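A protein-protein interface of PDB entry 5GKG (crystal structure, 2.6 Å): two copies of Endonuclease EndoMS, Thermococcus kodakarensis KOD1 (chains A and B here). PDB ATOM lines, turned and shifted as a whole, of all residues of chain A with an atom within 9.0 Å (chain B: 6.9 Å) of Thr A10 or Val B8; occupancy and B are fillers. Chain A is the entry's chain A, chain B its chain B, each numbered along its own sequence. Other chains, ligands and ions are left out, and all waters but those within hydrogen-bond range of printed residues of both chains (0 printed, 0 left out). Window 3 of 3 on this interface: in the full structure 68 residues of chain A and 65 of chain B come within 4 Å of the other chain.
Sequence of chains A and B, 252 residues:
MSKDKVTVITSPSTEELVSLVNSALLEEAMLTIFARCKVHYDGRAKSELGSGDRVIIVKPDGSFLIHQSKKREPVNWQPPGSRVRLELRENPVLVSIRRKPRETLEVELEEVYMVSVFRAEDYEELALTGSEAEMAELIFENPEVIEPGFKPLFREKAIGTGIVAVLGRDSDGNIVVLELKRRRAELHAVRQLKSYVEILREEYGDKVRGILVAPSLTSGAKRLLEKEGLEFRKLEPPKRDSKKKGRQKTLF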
ATOM      1  N   VAL A   6       2.122  24.825  -8.637  1.00  0.00           N
ATOM      2  CA  VAL A   6       0.939  25.143  -9.426  1.00  0.00           C
ATOM      3  C   VAL A   6      -0.343  24.674  -8.766  1.00  0.00           C
ATOM      4  O   VAL A   6      -0.446  23.549  -8.295  1.00  0.00           O
ATOM      5  CB  VAL A   6       1.001  24.509 -10.855  1.00  0.00           C
ATOM      6  CG1 VAL A   6      -0.315  24.715 -11.616  1.00  0.00           C
ATOM      7  CG2 VAL A   6       2.173  25.063 -11.646  1.00  0.00           C
ATOM      8  N   THR A   7      -1.324  25.563  -8.774  1.00  0.00           N
ATOM      9  CA  THR A   7      -2.681  25.277  -8.375  1.00  0.00           C
ATOM     10  C   THR A   7      -3.613  25.618  -9.552  1.00  0.00           C
ATOM     11  O   THR A   7      -3.486  26.679 -10.134  1.00  0.00           O
ATOM     12  CB  THR A   7      -3.076  26.106  -7.142  1.00  0.00           C
ATOM     13  OG1 THR A   7      -2.081  25.967  -6.113  1.00  0.00           O
ATOM     14  CG2 THR A   7      -4.461  25.697  -6.638  1.00  0.00           C
ATOM     15  N   VAL A   8      -4.552  24.738  -9.875  1.00  0.00           N
ATOM     16  CA  VAL A   8      -5.424  24.875 -11.030  1.00  0.00           C
ATOM     17  C   VAL A   8      -6.848  24.560 -10.601  1.00  0.00           C
ATOM     18  O   VAL A   8      -7.086  23.503 -10.034  1.00  0.00           O
ATOM     19  CB  VAL A   8      -5.025  23.885 -12.193  1.00  0.00           C
ATOM     20  CG1 VAL A   8      -6.012  23.958 -13.316  1.00  0.00           C
ATOM     21  CG2 VAL A   8      -3.648  24.166 -12.702  1.00  0.00           C
ATOM     22  N   ILE A   9      -7.795  25.445 -10.883  1.00  0.00           N
ATOM     23  CA  ILE A   9      -9.198  25.101 -10.719  1.00  0.00           C
ATOM     24  C   ILE A   9      -9.972  25.435 -11.996  1.00  0.00           C
ATOM     25  O   ILE A   9     -10.003  26.592 -12.439  1.00  0.00           O
ATOM     26  CB  ILE A   9      -9.842  25.841  -9.525  1.00  0.00           C
ATOM     27  CG1 ILE A   9      -9.054  25.605  -8.240  1.00  0.00           C
ATOM     28  CG2 ILE A   9     -11.278  25.383  -9.297  1.00  0.00           C
ATOM     29  CD1 ILE A   9      -9.763  26.152  -7.019  1.00  0.00           C
ATOM     30  N   THR A  10     -10.588  24.421 -12.599  1.00  0.00           N
ATOM     31  CA  THR A  10     -11.456  24.638 -13.761  1.00  0.00           C
ATOM     32  C   THR A  10     -12.860  24.912 -13.293  1.00  0.00           C
ATOM     33  O   THR A  10     -13.273  24.387 -12.280  1.00  0.00           O
ATOM     34  CB  THR A  10     -11.447  23.438 -14.730  1.00  0.00           C
ATOM     35  OG1 THR A  10     -11.804  22.241 -14.027  1.00  0.00           O
ATOM     36  CG2 THR A  10     -10.052  23.270 -15.338  1.00  0.00           C
ATOM     37  N   SER A  11     -13.577  25.768 -14.010  1.00  0.00           N
ATOM     38  CA  SER A  11     -14.909  26.203 -13.604  1.00  0.00           C
ATOM     39  C   SER A  11     -15.005  26.581 -12.116  1.00  0.00           C
ATOM     40  O   SER A  11     -15.814  26.008 -11.390  1.00  0.00           O
ATOM     41  CB  SER A  11     -15.934  25.103 -13.898  1.00  0.00           C
ATOM     42  OG  SER A  11     -15.826  24.602 -15.215  1.00  0.00           O
ATOM     43  N   PRO A  12     -14.181  27.536 -11.652  1.00  0.00           N
ATOM     44  CA  PRO A  12     -14.226  27.841 -10.214  1.00  0.00           C
ATOM     45  C   PRO A  12     -15.551  28.457  -9.766  1.00  0.00           C
ATOM     46  O   PRO A  12     -16.262  29.031 -10.579  1.00  0.00           O
ATOM     47  CB  PRO A  12     -13.076  28.840 -10.027  1.00  0.00           C
ATOM     48  CG  PRO A  12     -12.877  29.458 -11.383  1.00  0.00           C
ATOM     49  CD  PRO A  12     -13.200  28.372 -12.372  1.00  0.00           C
ATOM     50  N   SER A  13     -15.889  28.303  -8.491  1.00  0.00           N
ATOM     51  CA  SER A  13     -16.948  29.100  -7.892  1.00  0.00           C
ATOM     52  C   SER A  13     -16.398  30.493  -7.656  1.00  0.00           C
ATOM     53  O   SER A  13     -15.188  30.719  -7.800  1.00  0.00           O
ATOM     54  CB  SER A  13     -17.395  28.503  -6.564  1.00  0.00           C
ATOM     55  OG  SER A  13     -16.299  28.496  -5.656  1.00  0.00           O
ATOM     56  N   GLU A  16     -14.045  30.117  -4.986  1.00  0.00           N
ATOM     57  CA  GLU A  16     -12.844  29.467  -5.521  1.00  0.00           C
ATOM     58  C   GLU A  16     -12.010  30.499  -6.264  1.00  0.00           C
ATOM     59  O   GLU A  16     -10.790  30.580  -6.085  1.00  0.00           O
ATOM     60  CB  GLU A  16     -13.212  28.307  -6.441  1.00  0.00           C
ATOM     61  CG  GLU A  16     -13.245  26.947  -5.746  1.00  0.00           C
ATOM     62  CD  GLU A  16     -13.944  25.866  -6.566  1.00  0.00           C
ATOM     63  OE1 GLU A  16     -14.760  26.213  -7.443  1.00  0.00           O
ATOM     64  OE2 GLU A  16     -13.681  24.663  -6.345  1.00  0.00           O
ATOM     65  N   LEU A  17     -12.699  31.319  -7.058  1.00  0.00           N
ATOM     66  CA  LEU A  17     -12.065  32.366  -7.853  1.00  0.00           C
ATOM     67  C   LEU A  17     -11.349  33.382  -7.000  1.00  0.00           C
ATOM     68  O   LEU A  17     -10.182  33.710  -7.260  1.00  0.00           O
ATOM     69  CB  LEU A  17     -13.101  33.080  -8.713  1.00  0.00           C
ATOM     70  CG  LEU A  17     -12.583  34.256  -9.532  1.00  0.00           C
ATOM     71  CD1 LEU A  17     -11.418  33.827 -10.367  1.00  0.00           C
ATOM     72  CD2 LEU A  17     -13.702  34.784 -10.412  1.00  0.00           C
ATOM     73  N   LEU A  20      -8.090  31.983  -5.165  1.00  0.00           N
ATOM     74  CA  LEU A  20      -6.846  31.828  -5.933  1.00  0.00           C
ATOM     75  C   LEU A  20      -6.267  33.172  -6.307  1.00  0.00           C
ATOM     76  O   LEU A  20      -5.050  33.392  -6.202  1.00  0.00           O
ATOM     77  CB  LEU A  20      -7.061  30.979  -7.187  1.00  0.00           C
ATOM     78  CG  LEU A  20      -7.331  29.501  -6.861  1.00  0.00           C
ATOM     79  CD1 LEU A  20      -7.038  28.575  -8.040  1.00  0.00           C
ATOM     80  CD2 LEU A  20      -6.519  29.094  -5.663  1.00  0.00           C
ATOM     81  N   PHE A  34      -8.392  31.727 -17.718  1.00  0.00           N
ATOM     82  CA  PHE A  34      -9.016  31.505 -19.017  1.00  0.00           C
ATOM     83  C   PHE A  34     -10.473  31.916 -18.873  1.00  0.00           C
ATOM     84  O   PHE A  34     -11.190  31.377 -18.032  1.00  0.00           O
ATOM     85  CB  PHE A  34      -8.912  30.035 -19.462  1.00  0.00           C
ATOM     86  CG  PHE A  34      -7.494  29.527 -19.658  1.00  0.00           C
ATOM     87  CD1 PHE A  34      -6.427  30.401 -19.880  1.00  0.00           C
ATOM     88  CD2 PHE A  34      -7.235  28.151 -19.639  1.00  0.00           C
ATOM     89  CE1 PHE A  34      -5.116  29.915 -20.084  1.00  0.00           C
ATOM     90  CE2 PHE A  34      -5.937  27.651 -19.822  1.00  0.00           C
ATOM     91  CZ  PHE A  34      -4.870  28.539 -20.046  1.00  0.00           C
ATOM     92  N   GLU A 111     -17.580  34.382 -17.613  1.00  0.00           N
ATOM     93  CA  GLU A 111     -17.355  32.996 -17.252  1.00  0.00           C
ATOM     94  C   GLU A 111     -15.891  32.667 -17.067  1.00  0.00           C
ATOM     95  O   GLU A 111     -15.113  32.784 -18.019  1.00  0.00           O
ATOM     96  CB  GLU A 111     -17.932  32.082 -18.318  1.00  0.00           C
ATOM     97  CG  GLU A 111     -17.691  30.626 -18.034  1.00  0.00           C
ATOM     98  CD  GLU A 111     -18.736  29.761 -18.696  1.00  0.00           C
ATOM     99  OE1 GLU A 111     -19.474  30.289 -19.559  1.00  0.00           O
ATOM    100  OE2 GLU A 111     -18.832  28.566 -18.348  1.00  0.00           O
ATOM    101  N   VAL A 112     -15.507  32.184 -15.896  1.00  0.00           N
ATOM    102  CA  VAL A 112     -14.126  31.740 -15.752  1.00  0.00           C
ATOM    103  C   VAL A 112     -13.959  30.232 -15.990  1.00  0.00           C
ATOM    104  O   VAL A 112     -14.339  29.400 -15.176  1.00  0.00           O
ATOM    105  CB  VAL A 112     -13.577  32.093 -14.385  1.00  0.00           C
ATOM    106  CG1 VAL A 112     -12.126  31.667 -14.277  1.00  0.00           C
ATOM    107  CG2 VAL A 112     -13.735  33.598 -14.137  1.00  0.00           C
ATOM    108  N   TYR A 113     -13.338  29.903 -17.110  1.00  0.00           N
ATOM    109  CA  TYR A 113     -13.109  28.522 -17.500  1.00  0.00           C
ATOM    110  C   TYR A 113     -12.000  27.889 -16.677  1.00  0.00           C
ATOM    111  O   TYR A 113     -12.025  26.701 -16.397  1.00  0.00           O
ATOM    112  CB  TYR A 113     -12.740  28.445 -18.980  1.00  0.00           C
ATOM    113  CG  TYR A 113     -13.710  29.119 -19.908  1.00  0.00           C
ATOM    114  CD1 TYR A 113     -15.069  28.776 -19.910  1.00  0.00           C
ATOM    115  CD2 TYR A 113     -13.270  30.082 -20.816  1.00  0.00           C
ATOM    116  CE1 TYR A 113     -15.972  29.397 -20.787  1.00  0.00           C
ATOM    117  CE2 TYR A 113     -14.166  30.712 -21.692  1.00  0.00           C
ATOM    118  CZ  TYR A 113     -15.505  30.367 -21.680  1.00  0.00           C
ATOM    119  OH  TYR A 113     -16.366  31.007 -22.551  1.00  0.00           O
ATOM    120  N   MET A 114     -10.995  28.679 -16.340  1.00  0.00           N
ATOM    121  CA  MET A 114      -9.902  28.209 -15.515  1.00  0.00           C
ATOM    122  C   MET A 114      -9.263  29.371 -14.780  1.00  0.00           C
ATOM    123  O   MET A 114      -9.187  30.474 -15.313  1.00  0.00           O
ATOM    124  CB  MET A 114      -8.848  27.507 -16.358  1.00  0.00           C
ATOM    125  CG  MET A 114      -7.842  26.773 -15.527  1.00  0.00           C
ATOM    126  SD  MET A 114      -6.371  26.348 -16.441  1.00  0.00           S
ATOM    127  CE  MET A 114      -5.445  27.865 -16.115  1.00  0.00           C
ATOM    128  N   VAL A 115      -8.797  29.109 -13.565  1.00  0.00           N
ATOM    129  CA  VAL A 115      -7.964  30.040 -12.834  1.00  0.00           C
ATOM    130  C   VAL A 115      -6.803  29.243 -12.265  1.00  0.00           C
ATOM    131  O   VAL A 115      -6.985  28.117 -11.807  1.00  0.00           O
ATOM    132  CB  VAL A 115      -8.743  30.774 -11.693  1.00  0.00           C
ATOM    133  CG1 VAL A 115      -9.465  29.788 -10.793  1.00  0.00           C
ATOM    134  CG2 VAL A 115      -7.797  31.626 -10.860  1.00  0.00           C
ATOM    135  N   SER A 116      -5.606  29.807 -12.307  1.00  0.00           N
ATOM    136  CA  SER A 116      -4.448  29.092 -11.792  1.00  0.00           C
ATOM    137  C   SER A 116      -3.430  30.011 -11.141  1.00  0.00           C
ATOM    138  O   SER A 116      -3.270  31.166 -11.529  1.00  0.00           O
ATOM    139  CB  SER A 116      -3.760  28.293 -12.912  1.00  0.00           C
ATOM    140  OG  SER A 116      -3.125  29.157 -13.852  1.00  0.00           O
ATOM    141  N   VAL B   6     -11.478  23.825 -21.904  1.00  0.00           N
ATOM    142  CA  VAL B   6     -10.159  23.673 -21.343  1.00  0.00           C
ATOM    143  C   VAL B   6      -9.834  22.210 -21.141  1.00  0.00           C
ATOM    144  O   VAL B   6     -10.712  21.392 -20.874  1.00  0.00           O
ATOM    145  CB  VAL B   6     -10.023  24.434 -20.012  1.00  0.00           C
ATOM    146  CG1 VAL B   6      -8.575  24.483 -19.576  1.00  0.00           C
ATOM    147  CG2 VAL B   6     -10.536  25.834 -20.183  1.00  0.00           C
ATOM    148  N   THR B   7      -8.562  21.885 -21.332  1.00  0.00           N
ATOM    149  CA  THR B   7      -8.056  20.604 -20.974  1.00  0.00           C
ATOM    150  C   THR B   7      -6.739  20.865 -20.275  1.00  0.00           C
ATOM    151  O   THR B   7      -5.831  21.414 -20.877  1.00  0.00           O
ATOM    152  CB  THR B   7      -7.894  19.678 -22.215  1.00  0.00           C
ATOM    153  OG1 THR B   7      -9.175  19.483 -22.837  1.00  0.00           O
ATOM    154  CG2 THR B   7      -7.329  18.315 -21.800  1.00  0.00           C
ATOM    155  N   VAL B   8      -6.652  20.479 -18.999  1.00  0.00           N
ATOM    156  CA  VAL B   8      -5.499  20.780 -18.161  1.00  0.00           C
ATOM    157  C   VAL B   8      -4.869  19.552 -17.567  1.00  0.00           C
ATOM    158  O   VAL B   8      -5.550  18.702 -17.019  1.00  0.00           O
ATOM    159  CB  VAL B   8      -5.857  21.643 -16.944  1.00  0.00           C
ATOM    160  CG1 VAL B   8      -4.637  22.416 -16.485  1.00  0.00           C
ATOM    161  CG2 VAL B   8      -7.012  22.513 -17.232  1.00  0.00           C
ATOM    162  N   ILE B   9      -3.557  19.499 -17.579  1.00  0.00           N
ATOM    163  CA  ILE B   9      -2.900  18.450 -16.870  1.00  0.00           C
ATOM    164  C   ILE B   9      -1.772  19.055 -16.053  1.00  0.00           C
ATOM    165  O   ILE B   9      -0.978  19.832 -16.566  1.00  0.00           O
ATOM    166  CB  ILE B   9      -2.392  17.379 -17.843  1.00  0.00           C
ATOM    167  CG1 ILE B   9      -3.589  16.713 -18.520  1.00  0.00           C
ATOM    168  CG2 ILE B   9      -1.551  16.346 -17.127  1.00  0.00           C
ATOM    169  CD1 ILE B   9      -3.219  15.587 -19.413  1.00  0.00           C
ATOM    170  N   THR B  10      -1.701  18.732 -14.765  1.00  0.00           N
ATOM    171  CA  THR B  10      -0.544  19.179 -14.008  1.00  0.00           C
ATOM    172  C   THR B  10       0.384  17.995 -13.897  1.00  0.00           C
ATOM    173  O   THR B  10      -0.051  16.855 -14.010  1.00  0.00           O
ATOM    174  CB  THR B  10      -0.899  19.760 -12.637  1.00  0.00           C
ATOM    175  OG1 THR B  10      -1.764  18.866 -11.936  1.00  0.00           O
ATOM    176  CG2 THR B  10      -1.598  21.077 -12.835  1.00  0.00           C
ATOM    177  N   LEU B  20      -1.368  16.588 -25.561  1.00  0.00           N
ATOM    178  CA  LEU B  20      -2.054  17.868 -25.450  1.00  0.00           C
ATOM    179  C   LEU B  20      -1.412  18.915 -26.355  1.00  0.00           C
ATOM    180  O   LEU B  20      -2.107  19.755 -26.932  1.00  0.00           O
ATOM    181  CB  LEU B  20      -2.076  18.359 -24.015  1.00  0.00           C
ATOM    182  CG  LEU B  20      -3.361  17.949 -23.319  1.00  0.00           C
ATOM    183  CD1 LEU B  20      -3.160  16.577 -22.846  1.00  0.00           C
ATOM    184  CD2 LEU B  20      -3.664  18.872 -22.153  1.00  0.00           C
ATOM    185  N   MET B 114       2.575  22.349 -15.831  1.00  0.00           N
ATOM    186  CA  MET B 114       1.222  22.292 -16.368  1.00  0.00           C
ATOM    187  C   MET B 114       1.206  22.412 -17.873  1.00  0.00           C
ATOM    188  O   MET B 114       2.029  23.117 -18.437  1.00  0.00           O
ATOM    189  CB  MET B 114       0.365  23.400 -15.763  1.00  0.00           C
ATOM    190  CG  MET B 114      -1.104  23.235 -16.046  1.00  0.00           C
ATOM    191  SD  MET B 114      -1.845  24.768 -16.568  1.00  0.00           S
ATOM    192  CE  MET B 114      -1.073  24.999 -18.137  1.00  0.00           C
ATOM    193  N   VAL B 115       0.268  21.726 -18.521  1.00  0.00           N
ATOM    194  CA  VAL B 115       0.032  21.917 -19.943  1.00  0.00           C
ATOM    195  C   VAL B 115      -1.458  21.992 -20.162  1.00  0.00           C
ATOM    196  O   VAL B 115      -2.206  21.228 -19.572  1.00  0.00           O
ATOM    197  CB  VAL B 115       0.636  20.803 -20.823  1.00  0.00           C
ATOM    198  CG1 VAL B 115       0.226  19.424 -20.320  1.00  0.00           C
ATOM    199  CG2 VAL B 115       0.225  21.017 -22.307  1.00  0.00           C
ATOM    200  N   SER B 116      -1.892  22.932 -20.998  1.00  0.00           N
ATOM    201  CA  SER B 116      -3.311  23.137 -21.186  1.00  0.00           C
ATOM    202  C   SER B 116      -3.634  23.517 -22.617  1.00  0.00           C
ATOM    203  O   SER B 116      -2.837  24.153 -23.324  1.00  0.00           O
ATOM    204  CB  SER B 116      -3.856  24.217 -20.219  1.00  0.00           C
ATOM    205  OG  SER B 116      -3.293  25.490 -20.498  1.00  0.00           O
ATOM    206  N   VAL B 117      -4.828  23.110 -23.017  1.00  0.00           N
ATOM    207  CA  VAL B 117      -5.433  23.503 -24.268  1.00  0.00           C
ATOM    208  C   VAL B 117      -6.661  24.342 -23.930  1.00  0.00           C
ATOM    209  O   VAL B 117      -7.506  23.944 -23.130  1.00  0.00           O
ATOM    210  CB  VAL B 117      -5.800  22.258 -25.128  1.00  0.00           C
ATOM    211  CG1 VAL B 117      -6.416  22.673 -26.431  1.00  0.00           C
ATOM    212  CG2 VAL B 117      -4.559  21.415 -25.365  1.00  0.00           C
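The backbone NH (N) of Ser A11 is in hydrogen-bond range of the backbone carbonyl oxygen (O) of Tyr A113, at 3.0 Å.
The backbone carbonyl oxygen (O) of Phe A34 sits at hydrogen-bond distance from the backbone NH (N) of Tyr A113, at 2.8 Å.
The backbone NH of Phe A34 sits at hydrogen-bond distance from the backbone carbonyl oxygen of Met A114.
Among the printed residues, merely in contact across the chains: Phe A34 with Ser B116, Tyr A113 with Val B6, Thr A10 with Val B8, Val A8 with Thr B10, Val A8 with Val B8, Phe A34 with Val B6 and Met A114 with Val B8.
Thr A10 touches one residue of chain B.
Of chain A, only Val A8 (3.8 Å), Thr A10 (3.7 Å) and Met A114 (3.97 Å) come within 4 Å of Val B8.
Thr B7 touches none of the printed residues of chain A.
No residue of chain A comes within 4 Å of Ile B9.
Printed residues of chain B within 4 Å of Phe A34: Val B6 (3.9 Å) and Ser B116 (3.5 Å).
Of the printed residues of chain A, Val B6 touches Phe A34 (3.9 Å) and Tyr A113 (3.6 Å).
Printed residues of chain A within 4 Å of Ser B116: Phe A34.
Printed residues of chain B within 4 Å of Tyr A113: Val B6.
The nearest residue of chain A that does not touch Val B8 is Phe A34 (5.9 Å).
The nearest printed residue of chain B that does not touch Val A8 is Met B114 (4.3 Å).
Val A8 touches its own counterpart, Val B8.
Val A8 touches Thr B10, and with the chains exchanged Thr A10 touches Val B8.
Met A114 touches Val B8, but with the chains exchanged Val A8 does not touch Met B114 (4.3 Å).
9 positions are printed for both chains.
Of the 7 pairs that touch across the chains among the printed residues, 3 have their exchanged pair printed and touching as well.
Of the 18 printed residues of chain A, 5 touch a printed residue of chain B.
Hydrophobic or aromatic side chains of chain A within 4 Å of the printed part of chain B: Val A8, Phe A34, Tyr A113 and Met A114.
Of the 10 printed residues of chain B, 4 touch a printed residue of chain A.
Hydrophobic or aromatic side chains of chain B within 4 Å of the printed part of chain A: Val B6 and Val B8.
Among the printed residues, 7 pairs touch across the chains.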
